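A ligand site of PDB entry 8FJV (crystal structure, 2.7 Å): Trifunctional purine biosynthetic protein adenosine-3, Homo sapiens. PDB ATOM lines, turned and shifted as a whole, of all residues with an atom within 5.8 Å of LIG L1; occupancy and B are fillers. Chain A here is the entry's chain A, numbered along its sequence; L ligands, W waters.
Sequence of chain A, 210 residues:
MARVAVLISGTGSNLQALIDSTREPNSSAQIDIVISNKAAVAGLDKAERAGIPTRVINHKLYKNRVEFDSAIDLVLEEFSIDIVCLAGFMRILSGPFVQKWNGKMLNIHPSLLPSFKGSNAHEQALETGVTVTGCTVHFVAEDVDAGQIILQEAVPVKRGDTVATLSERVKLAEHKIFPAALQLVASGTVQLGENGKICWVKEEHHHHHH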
ATOM      1  N   HIS A  59     -17.049 -18.938 -23.016  1.00  0.00           N
ATOM      2  CA  HIS A  59     -15.965 -18.099 -22.533  1.00  0.00           C
ATOM      3  C   HIS A  59     -16.407 -16.665 -22.338  1.00  0.00           C
ATOM      4  O   HIS A  59     -15.856 -15.953 -21.500  1.00  0.00           O
ATOM      5  CB  HIS A  59     -14.782 -18.167 -23.501  1.00  0.00           C
ATOM      6  CG  HIS A  59     -15.088 -17.615 -24.861  1.00  0.00           C
ATOM      7  ND1 HIS A  59     -15.797 -18.332 -25.800  1.00  0.00           N
ATOM      8  CD2 HIS A  59     -14.789 -16.430 -25.429  1.00  0.00           C
ATOM      9  CE1 HIS A  59     -15.921 -17.607 -26.894  1.00  0.00           C
ATOM     10  NE2 HIS A  59     -15.306 -16.450 -26.699  1.00  0.00           N
ATOM     11  N   ARG A  65     -10.337 -15.610 -17.479  1.00  0.00           N
ATOM     12  CA  ARG A  65      -9.970 -16.753 -18.315  1.00  0.00           C
ATOM     13  C   ARG A  65      -9.823 -18.010 -17.468  1.00  0.00           C
ATOM     14  O   ARG A  65     -10.186 -19.105 -17.912  1.00  0.00           O
ATOM     15  CB  ARG A  65      -8.675 -16.450 -19.072  1.00  0.00           C
ATOM     16  CG  ARG A  65      -8.293 -17.467 -20.137  1.00  0.00           C
ATOM     17  CD  ARG A  65      -7.016 -17.069 -20.864  1.00  0.00           C
ATOM     18  NE  ARG A  65      -7.147 -15.841 -21.646  1.00  0.00           N
ATOM     19  CZ  ARG A  65      -7.211 -15.776 -22.974  1.00  0.00           C
ATOM     20  NH1 ARG A  65      -7.145 -16.872 -23.724  1.00  0.00           N
ATOM     21  NH2 ARG A  65      -7.330 -14.595 -23.583  1.00  0.00           N
ATOM     22  N   LEU A  86      -7.739 -30.947 -28.523  1.00  0.00           N
ATOM     23  CA  LEU A  86      -8.193 -29.673 -29.076  1.00  0.00           C
ATOM     24  C   LEU A  86      -8.362 -29.844 -30.590  1.00  0.00           C
ATOM     25  O   LEU A  86      -7.393 -30.081 -31.304  1.00  0.00           O
ATOM     26  CB  LEU A  86      -7.194 -28.569 -28.749  1.00  0.00           C
ATOM     27  CG  LEU A  86      -6.922 -28.362 -27.262  1.00  0.00           C
ATOM     28  CD1 LEU A  86      -5.959 -27.194 -27.045  1.00  0.00           C
ATOM     29  CD2 LEU A  86      -8.221 -28.138 -26.485  1.00  0.00           C
ATOM     30  N   PHE A  89     -10.241 -25.581 -31.479  1.00  0.00           N
ATOM     31  CA  PHE A  89     -10.600 -24.842 -30.283  1.00  0.00           C
ATOM     32  C   PHE A  89      -9.840 -23.522 -30.288  1.00  0.00           C
ATOM     33  O   PHE A  89      -8.599 -23.519 -30.249  1.00  0.00           O
ATOM     34  CB  PHE A  89     -10.270 -25.662 -29.054  1.00  0.00           C
ATOM     35  CG  PHE A  89     -10.790 -25.093 -27.790  1.00  0.00           C
ATOM     36  CD1 PHE A  89     -12.148 -25.132 -27.510  1.00  0.00           C
ATOM     37  CD2 PHE A  89      -9.916 -24.549 -26.846  1.00  0.00           C
ATOM     38  CE1 PHE A  89     -12.638 -24.615 -26.315  1.00  0.00           C
ATOM     39  CE2 PHE A  89     -10.382 -24.037 -25.651  1.00  0.00           C
ATOM     40  CZ  PHE A  89     -11.758 -24.061 -25.378  1.00  0.00           C
ATOM     41  N   MET A  90     -10.574 -22.402 -30.317  1.00  0.00           N
ATOM     42  CA  MET A  90      -9.994 -21.080 -30.528  1.00  0.00           C
ATOM     43  C   MET A  90      -9.989 -20.235 -29.253  1.00  0.00           C
ATOM     44  O   MET A  90     -10.302 -19.050 -29.288  1.00  0.00           O
ATOM     45  CB  MET A  90     -10.722 -20.332 -31.645  1.00  0.00           C
ATOM     46  CG  MET A  90     -10.871 -21.104 -32.948  1.00  0.00           C
ATOM     47  SD  MET A  90      -9.319 -21.670 -33.690  1.00  0.00           S
ATOM     48  CE  MET A  90      -9.906 -22.288 -35.264  1.00  0.00           C
ATOM     49  N   ARG A  91      -9.625 -20.828 -28.127  1.00  0.00           N
ATOM     50  CA  ARG A  91      -9.467 -20.086 -26.878  1.00  0.00           C
ATOM     51  C   ARG A  91      -8.154 -20.494 -26.239  1.00  0.00           C
ATOM     52  O   ARG A  91      -7.882 -21.690 -26.075  1.00  0.00           O
ATOM     53  CB  ARG A  91     -10.623 -20.347 -25.917  1.00  0.00           C
ATOM     54  CG  ARG A  91     -11.951 -19.805 -26.387  1.00  0.00           C
ATOM     55  CD  ARG A  91     -11.879 -18.310 -26.620  1.00  0.00           C
ATOM     56  NE  ARG A  91     -11.077 -17.639 -25.597  1.00  0.00           N
ATOM     57  CZ  ARG A  91     -11.030 -16.320 -25.434  1.00  0.00           C
ATOM     58  NH1 ARG A  91     -10.270 -15.788 -24.477  1.00  0.00           N
ATOM     59  NH2 ARG A  91     -11.748 -15.520 -26.214  1.00  0.00           N
ATOM     60  N   ILE A  92      -7.337 -19.516 -25.869  1.00  0.00           N
ATOM     61  CA  ILE A  92      -6.065 -19.811 -25.243  1.00  0.00           C
ATOM     62  C   ILE A  92      -6.298 -20.174 -23.784  1.00  0.00           C
ATOM     63  O   ILE A  92      -7.040 -19.485 -23.073  1.00  0.00           O
ATOM     64  CB  ILE A  92      -5.090 -18.625 -25.382  1.00  0.00           C
ATOM     65  CG1 ILE A  92      -4.874 -18.301 -26.852  1.00  0.00           C
ATOM     66  CG2 ILE A  92      -3.746 -18.991 -24.804  1.00  0.00           C
ATOM     67  CD1 ILE A  92      -4.454 -19.514 -27.685  1.00  0.00           C
ATOM     68  N   LEU A  93      -5.694 -21.261 -23.349  1.00  0.00           N
ATOM     69  CA  LEU A  93      -5.903 -21.743 -21.996  1.00  0.00           C
ATOM     70  C   LEU A  93      -4.880 -21.140 -21.054  1.00  0.00           C
ATOM     71  O   LEU A  93      -3.756 -20.840 -21.442  1.00  0.00           O
ATOM     72  CB  LEU A  93      -5.841 -23.274 -21.957  1.00  0.00           C
ATOM     73  CG  LEU A  93      -6.972 -23.866 -22.789  1.00  0.00           C
ATOM     74  CD1 LEU A  93      -6.558 -25.166 -23.474  1.00  0.00           C
ATOM     75  CD2 LEU A  93      -8.206 -24.065 -21.907  1.00  0.00           C
ATOM     76  N   SER A  94      -5.293 -20.958 -19.796  1.00  0.00           N
ATOM     77  CA  SER A  94      -4.442 -20.351 -18.791  1.00  0.00           C
ATOM     78  C   SER A  94      -3.344 -21.316 -18.347  1.00  0.00           C
ATOM     79  O   SER A  94      -3.418 -22.532 -18.551  1.00  0.00           O
ATOM     80  CB  SER A  94      -5.262 -19.904 -17.578  1.00  0.00           C
ATOM     81  OG  SER A  94      -5.589 -21.010 -16.745  1.00  0.00           O
ATOM     82  N   VAL A  98      -3.064 -25.499 -18.495  1.00  0.00           N
ATOM     83  CA  VAL A  98      -2.097 -26.150 -19.380  1.00  0.00           C
ATOM     84  C   VAL A  98      -1.098 -26.963 -18.581  1.00  0.00           C
ATOM     85  O   VAL A  98      -0.684 -28.047 -18.983  1.00  0.00           O
ATOM     86  CB  VAL A  98      -1.387 -25.099 -20.259  1.00  0.00           C
ATOM     87  CG1 VAL A  98      -0.269 -25.755 -21.050  1.00  0.00           C
ATOM     88  CG2 VAL A  98      -2.396 -24.406 -21.177  1.00  0.00           C
ATOM     89  N   ASN A 107      -3.077 -31.027 -29.569  1.00  0.00           N
ATOM     90  CA  ASN A 107      -3.593 -30.009 -30.464  1.00  0.00           C
ATOM     91  C   ASN A 107      -3.225 -30.315 -31.911  1.00  0.00           C
ATOM     92  O   ASN A 107      -2.144 -30.836 -32.185  1.00  0.00           O
ATOM     93  CB  ASN A 107      -3.051 -28.636 -30.089  1.00  0.00           C
ATOM     94  CG  ASN A 107      -3.706 -27.534 -30.857  1.00  0.00           C
ATOM     95  OD1 ASN A 107      -4.868 -27.207 -30.624  1.00  0.00           O
ATOM     96  ND2 ASN A 107      -2.970 -26.940 -31.791  1.00  0.00           N
ATOM     97  N   GLY A 118       0.363 -19.700 -34.922  1.00  0.00           N
ATOM     98  CA  GLY A 118      -0.697 -18.734 -34.786  1.00  0.00           C
ATOM     99  C   GLY A 118      -1.916 -19.124 -35.594  1.00  0.00           C
ATOM    100  O   GLY A 118      -2.038 -20.231 -36.123  1.00  0.00           O
ATOM    101  N   SER A 119      -2.825 -18.164 -35.704  1.00  0.00           N
ATOM    102  CA  SER A 119      -4.195 -18.467 -36.065  1.00  0.00           C
ATOM    103  C   SER A 119      -4.436 -18.498 -37.558  1.00  0.00           C
ATOM    104  O   SER A 119      -5.356 -19.185 -38.015  1.00  0.00           O
ATOM    105  CB  SER A 119      -5.123 -17.468 -35.390  1.00  0.00           C
ATOM    106  OG  SER A 119      -4.360 -16.309 -35.108  1.00  0.00           O
ATOM    107  N   HIS A 138       0.692 -31.901 -31.699  1.00  0.00           N
ATOM    108  CA  HIS A 138       1.687 -31.663 -30.674  1.00  0.00           C
ATOM    109  C   HIS A 138       1.039 -31.674 -29.295  1.00  0.00           C
ATOM    110  O   HIS A 138      -0.189 -31.630 -29.153  1.00  0.00           O
ATOM    111  CB  HIS A 138       2.405 -30.335 -30.913  1.00  0.00           C
ATOM    112  CG  HIS A 138       1.499 -29.143 -30.904  1.00  0.00           C
ATOM    113  ND1 HIS A 138       1.434 -28.248 -29.857  1.00  0.00           N
ATOM    114  CD2 HIS A 138       0.603 -28.702 -31.830  1.00  0.00           C
ATOM    115  CE1 HIS A 138       0.546 -27.311 -30.129  1.00  0.00           C
ATOM    116  NE2 HIS A 138       0.031 -27.567 -31.320  1.00  0.00           N
ATOM    117  N   VAL A 140       0.128 -29.608 -26.034  1.00  0.00           N
ATOM    118  CA  VAL A 140      -0.047 -28.221 -25.612  1.00  0.00           C
ATOM    119  C   VAL A 140       0.921 -27.881 -24.480  1.00  0.00           C
ATOM    120  O   VAL A 140       0.966 -28.561 -23.449  1.00  0.00           O
ATOM    121  CB  VAL A 140      -1.490 -27.973 -25.200  1.00  0.00           C
ATOM    122  CG1 VAL A 140      -1.727 -26.486 -24.875  1.00  0.00           C
ATOM    123  CG2 VAL A 140      -2.432 -28.439 -26.296  1.00  0.00           C
ATOM    124  N   ALA A 141       1.716 -26.843 -24.687  1.00  0.00           N
ATOM    125  CA  ALA A 141       2.599 -26.284 -23.680  1.00  0.00           C
ATOM    126  C   ALA A 141       2.240 -24.812 -23.477  1.00  0.00           C
ATOM    127  O   ALA A 141       1.451 -24.244 -24.239  1.00  0.00           O
ATOM    128  CB  ALA A 141       4.065 -26.437 -24.107  1.00  0.00           C
ATOM    129  N   GLU A 142       2.802 -24.194 -22.434  1.00  0.00           N
ATOM    130  CA  GLU A 142       2.433 -22.807 -22.133  1.00  0.00           C
ATOM    131  C   GLU A 142       2.788 -21.860 -23.268  1.00  0.00           C
ATOM    132  O   GLU A 142       2.102 -20.843 -23.454  1.00  0.00           O
ATOM    133  CB  GLU A 142       3.062 -22.370 -20.817  1.00  0.00           C
ATOM    134  CG  GLU A 142       2.193 -22.723 -19.619  1.00  0.00           C
ATOM    135  CD  GLU A 142       2.783 -22.317 -18.271  1.00  0.00           C
ATOM    136  OE1 GLU A 142       3.528 -21.326 -18.225  1.00  0.00           O
ATOM    137  OE2 GLU A 142       2.492 -23.009 -17.255  1.00  0.00           O
ATOM    138  N   ASP A 143       3.832 -22.152 -24.045  1.00  0.00           N
ATOM    139  CA  ASP A 143       4.107 -21.409 -25.284  1.00  0.00           C
ATOM    140  C   ASP A 143       3.166 -21.898 -26.371  1.00  0.00           C
ATOM    141  O   ASP A 143       3.231 -23.061 -26.769  1.00  0.00           O
ATOM    142  CB  ASP A 143       5.555 -21.571 -25.724  1.00  0.00           C
ATOM    143  CG  ASP A 143       6.521 -20.826 -24.846  1.00  0.00           C
ATOM    144  OD1 ASP A 143       7.420 -21.470 -24.261  1.00  0.00           O
ATOM    145  OD2 ASP A 143       6.364 -19.593 -24.705  1.00  0.00           O
ATOM    146  N   VAL A 144       2.294 -21.004 -26.861  1.00  0.00           N
ATOM    147  CA  VAL A 144       1.311 -21.391 -27.877  1.00  0.00           C
ATOM    148  C   VAL A 144       2.017 -21.929 -29.114  1.00  0.00           C
ATOM    149  O   VAL A 144       2.939 -21.301 -29.652  1.00  0.00           O
ATOM    150  CB  VAL A 144       0.387 -20.209 -28.207  1.00  0.00           C
ATOM    151  CG1 VAL A 144      -0.578 -20.556 -29.346  1.00  0.00           C
ATOM    152  CG2 VAL A 144      -0.387 -19.787 -26.966  1.00  0.00           C
ATOM    153  N   ASP A 145       1.576 -23.099 -29.570  1.00  0.00           N
ATOM    154  CA  ASP A 145       2.167 -23.875 -30.667  1.00  0.00           C
ATOM    155  C   ASP A 145       3.641 -24.216 -30.436  1.00  0.00           C
ATOM    156  O   ASP A 145       4.315 -24.660 -31.366  1.00  0.00           O
ATOM    157  CB  ASP A 145       1.991 -23.172 -32.028  1.00  0.00           C
ATOM    158  CG  ASP A 145       0.533 -22.940 -32.408  1.00  0.00           C
ATOM    159  OD1 ASP A 145      -0.354 -23.749 -32.057  1.00  0.00           O
ATOM    160  OD2 ASP A 145       0.256 -21.926 -33.056  1.00  0.00           O
ATOM    161  N   ALA A 146       4.156 -24.030 -29.219  1.00  0.00           N
ATOM    162  CA  ALA A 146       5.540 -24.376 -28.899  1.00  0.00           C
ATOM    163  C   ALA A 146       5.598 -25.532 -27.907  1.00  0.00           C
ATOM    164  O   ALA A 146       6.314 -25.461 -26.910  1.00  0.00           O
ATOM    165  CB  ALA A 146       6.296 -23.160 -28.351  1.00  0.00           C
HETATM  166  C1  LIG L   1      -3.698 -19.984 -31.773  1.00  0.00           C
HETATM  167  C2  LIG L   1      -6.033 -16.936 -30.414  1.00  0.00           C
HETATM  168  C3  LIG L   1      -7.716 -15.837 -28.888  1.00  0.00           C
HETATM  169  C4  LIG L   1      -5.000 -20.451 -31.551  1.00  0.00           C
HETATM  170  C5  LIG L   1      -3.923 -22.875 -25.843  1.00  0.00           C
HETATM  171  C6  LIG L   1      -5.503 -23.358 -27.396  1.00  0.00           C
HETATM  172  O1  LIG L   1      -5.752 -15.894 -30.886  1.00  0.00           O
HETATM  173  C7  LIG L   1      -5.913 -19.463 -31.067  1.00  0.00           C
HETATM  174  C8  LIG L   1      -1.927 -23.634 -26.971  1.00  0.00           C
HETATM  175  C9  LIG L   1      -1.823 -22.708 -24.847  1.00  0.00           C
HETATM  176  C10 LIG L   1      -5.317 -22.819 -26.121  1.00  0.00           C
HETATM  177  C11 LIG L   1      -3.340 -23.439 -26.953  1.00  0.00           C
HETATM  178  C12 LIG L   1      -5.327 -18.196 -30.907  1.00  0.00           C
HETATM  179  C13 LIG L   1      -9.204 -15.985 -29.142  1.00  0.00           C
HETATM  180  C14 LIG L   1      -9.594 -15.825 -30.606  1.00  0.00           C
HETATM  181  C15 LIG L   1     -11.084 -16.079 -30.782  1.00  0.00           C
HETATM  182  C16 LIG L   1      -7.542 -15.680 -27.387  1.00  0.00           C
HETATM  183  C17 LIG L   1      -4.042 -24.312 -29.144  1.00  0.00           C
HETATM  184  C18 LIG L   1      -3.976 -23.195 -30.181  1.00  0.00           C
HETATM  185  C19 LIG L   1      -5.387 -22.714 -30.502  1.00  0.00           C
HETATM  186  C20 LIG L   1      -5.423 -21.896 -31.791  1.00  0.00           C
HETATM  187  F1  LIG L   1      -7.223 -19.681 -30.777  1.00  0.00           F
HETATM  188  N1  LIG L   1      -3.136 -22.513 -24.790  1.00  0.00           N
HETATM  189  N2  LIG L   1      -1.211 -23.256 -25.903  1.00  0.00           N
HETATM  190  N3  LIG L   1      -4.320 -23.718 -27.855  1.00  0.00           N
HETATM  191  N4  LIG L   1      -1.023 -22.311 -23.705  1.00  0.00           N
HETATM  192  N5  LIG L   1      -7.045 -17.019 -29.371  1.00  0.00           N
HETATM  193  O2  LIG L   1      -1.320 -24.203 -28.096  1.00  0.00           O
HETATM  194  O3  LIG L   1     -11.574 -16.473 -32.027  1.00  0.00           O
HETATM  195  O4  LIG L   1     -11.944 -15.928 -29.682  1.00  0.00           O
HETATM  196  O5  LIG L   1      -8.014 -16.679 -26.528  1.00  0.00           O
HETATM  197  O6  LIG L   1      -6.924 -14.528 -26.858  1.00  0.00           O
HETATM  198  S1  LIG L   1      -3.711 -18.346 -31.368  1.00  0.00           S
HETATM  199  C1  LG2 L   2      -8.212 -27.115 -38.542  1.00  0.00           C
HETATM  200  O1  LG2 L   2      -8.123 -26.790 -39.943  1.00  0.00           O
HETATM  201  C2  LG2 L   2      -6.908 -26.708 -37.838  1.00  0.00           C
HETATM  202  O2  LG2 L   2      -5.797 -26.750 -38.727  1.00  0.00           O
HETATM  203  C3  LG2 L   2      -7.284 -25.319 -37.288  1.00  0.00           C
HETATM  204  O3  LG2 L   2      -8.738 -25.352 -37.112  1.00  0.00           O
HETATM  205  C4  LG2 L   2      -9.400 -26.353 -37.933  1.00  0.00           C
HETATM  206  C5  LG2 L   2     -10.459 -27.246 -37.265  1.00  0.00           C
HETATM  207  O4  LG2 L   2     -11.374 -27.734 -38.269  1.00  0.00           O
HETATM  208  N1  LG2 L   2      -6.554 -24.837 -36.129  1.00  0.00           N
HETATM  209  C6  LG2 L   2      -6.258 -23.530 -36.109  1.00  0.00           C
HETATM  210  O5  LG2 L   2      -6.614 -22.718 -36.967  1.00  0.00           O
HETATM  211  C7  LG2 L   2      -5.461 -23.070 -34.915  1.00  0.00           C
HETATM  212  N2  LG2 L   2      -4.679 -21.894 -35.209  1.00  0.00           N
HETATM  213  P1  LG2 L   2     -12.673 -28.627 -37.918  1.00  0.00           P
HETATM  214  O6  LG2 L   2     -12.101 -29.846 -37.196  1.00  0.00           O
HETATM  215  O7  LG2 L   2     -13.503 -27.721 -37.049  1.00  0.00           O
HETATM  216  O8  LG2 L   2     -13.363 -28.929 -39.233  1.00  0.00           O
HETATM  217  O   HOH W   1       1.252 -25.303 -27.187  1.00  0.00           O
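Water W1 lies within hydrogen-bond range of an oxygen (O2) of LIG L1 (2.9 Å), the backbone NH (N) of Ala 141 (3.0 Å), the backbone carbonyl oxygen (O) of Asp 143 (3.0 Å) and the backbone NH (N) of Asp 145 (3.3 Å).
A fluorine (F1) of LIG L1 lies close to the backbone carbonyl oxygen (O) of Met 90 (3.5 Å).
Leu 86 touches LIG L1 (CD1 to C6, 3.9 Å).
O of Phe 89 touches C19 of LIG L1 (3.3 Å).
Val 98 touches LIG L1 (CG2 to N4, 3.6 Å).
Asn 107 touches LIG L1.
Val 140 touches LIG L1.
CA of Val 144 touches N2 of LIG L1 (3.7 Å).
Hydrophobic or aromatic side chains that line LIG L1: Leu 86, Met 90, Ile 92, Leu 93, Val 98, Val 140 and Val 144.
14 residues have an atom within 4 Å of LIG L1: Arg 65, Leu 86, Phe 89, Met 90, Arg 91, Ile 92, Leu 93, Val 98, Asn 107, Val 140, Ala 141, Glu 142, Val 144 and Asp 145.
O5 of LIG L1 lies within salt-bridge range of NH1 of Arg 91, at 3.2 Å.
O5 of LIG L1 is in salt-bridge range of NH1 of Arg 65, at 2.9 Å.
The backbone NH (N) of Ile 92 is in hydrogen-bond range of an oxygen (O5) of LIG L1, at 3.0 Å.
The backbone carbonyl oxygen (O) of Ala 141 sits at hydrogen-bond distance from a nitrogen (N4) of LIG L1, at 3.2 Å.
The backbone NH (N) of Leu 93 sits at hydrogen-bond distance from a nitrogen (N1) of LIG L1 (3.2 Å).
N of Asp 145 sits at hydrogen-bond distance from O2 of LIG L1 (3.4 Å).
N4 of LIG L1 lies within hydrogen-bond range of O of Glu 142.
O of Gly 118 sits at hydrogen-bond distance from N2 of LG2 L2 (3.3 Å).
The backbone carbonyl oxygen (O) of Ile 92 is in hydrogen-bond range of the guanidinium group (NH1) of Arg 65, at 2.7 Å.
The backbone NH (N) of Asn 107 is in hydrogen-bond range of the backbone carbonyl oxygen (O) of His 138 (3.0 Å).
N of Gly 118 sits at hydrogen-bond distance from OD2 of Asp 145 (2.9 Å).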
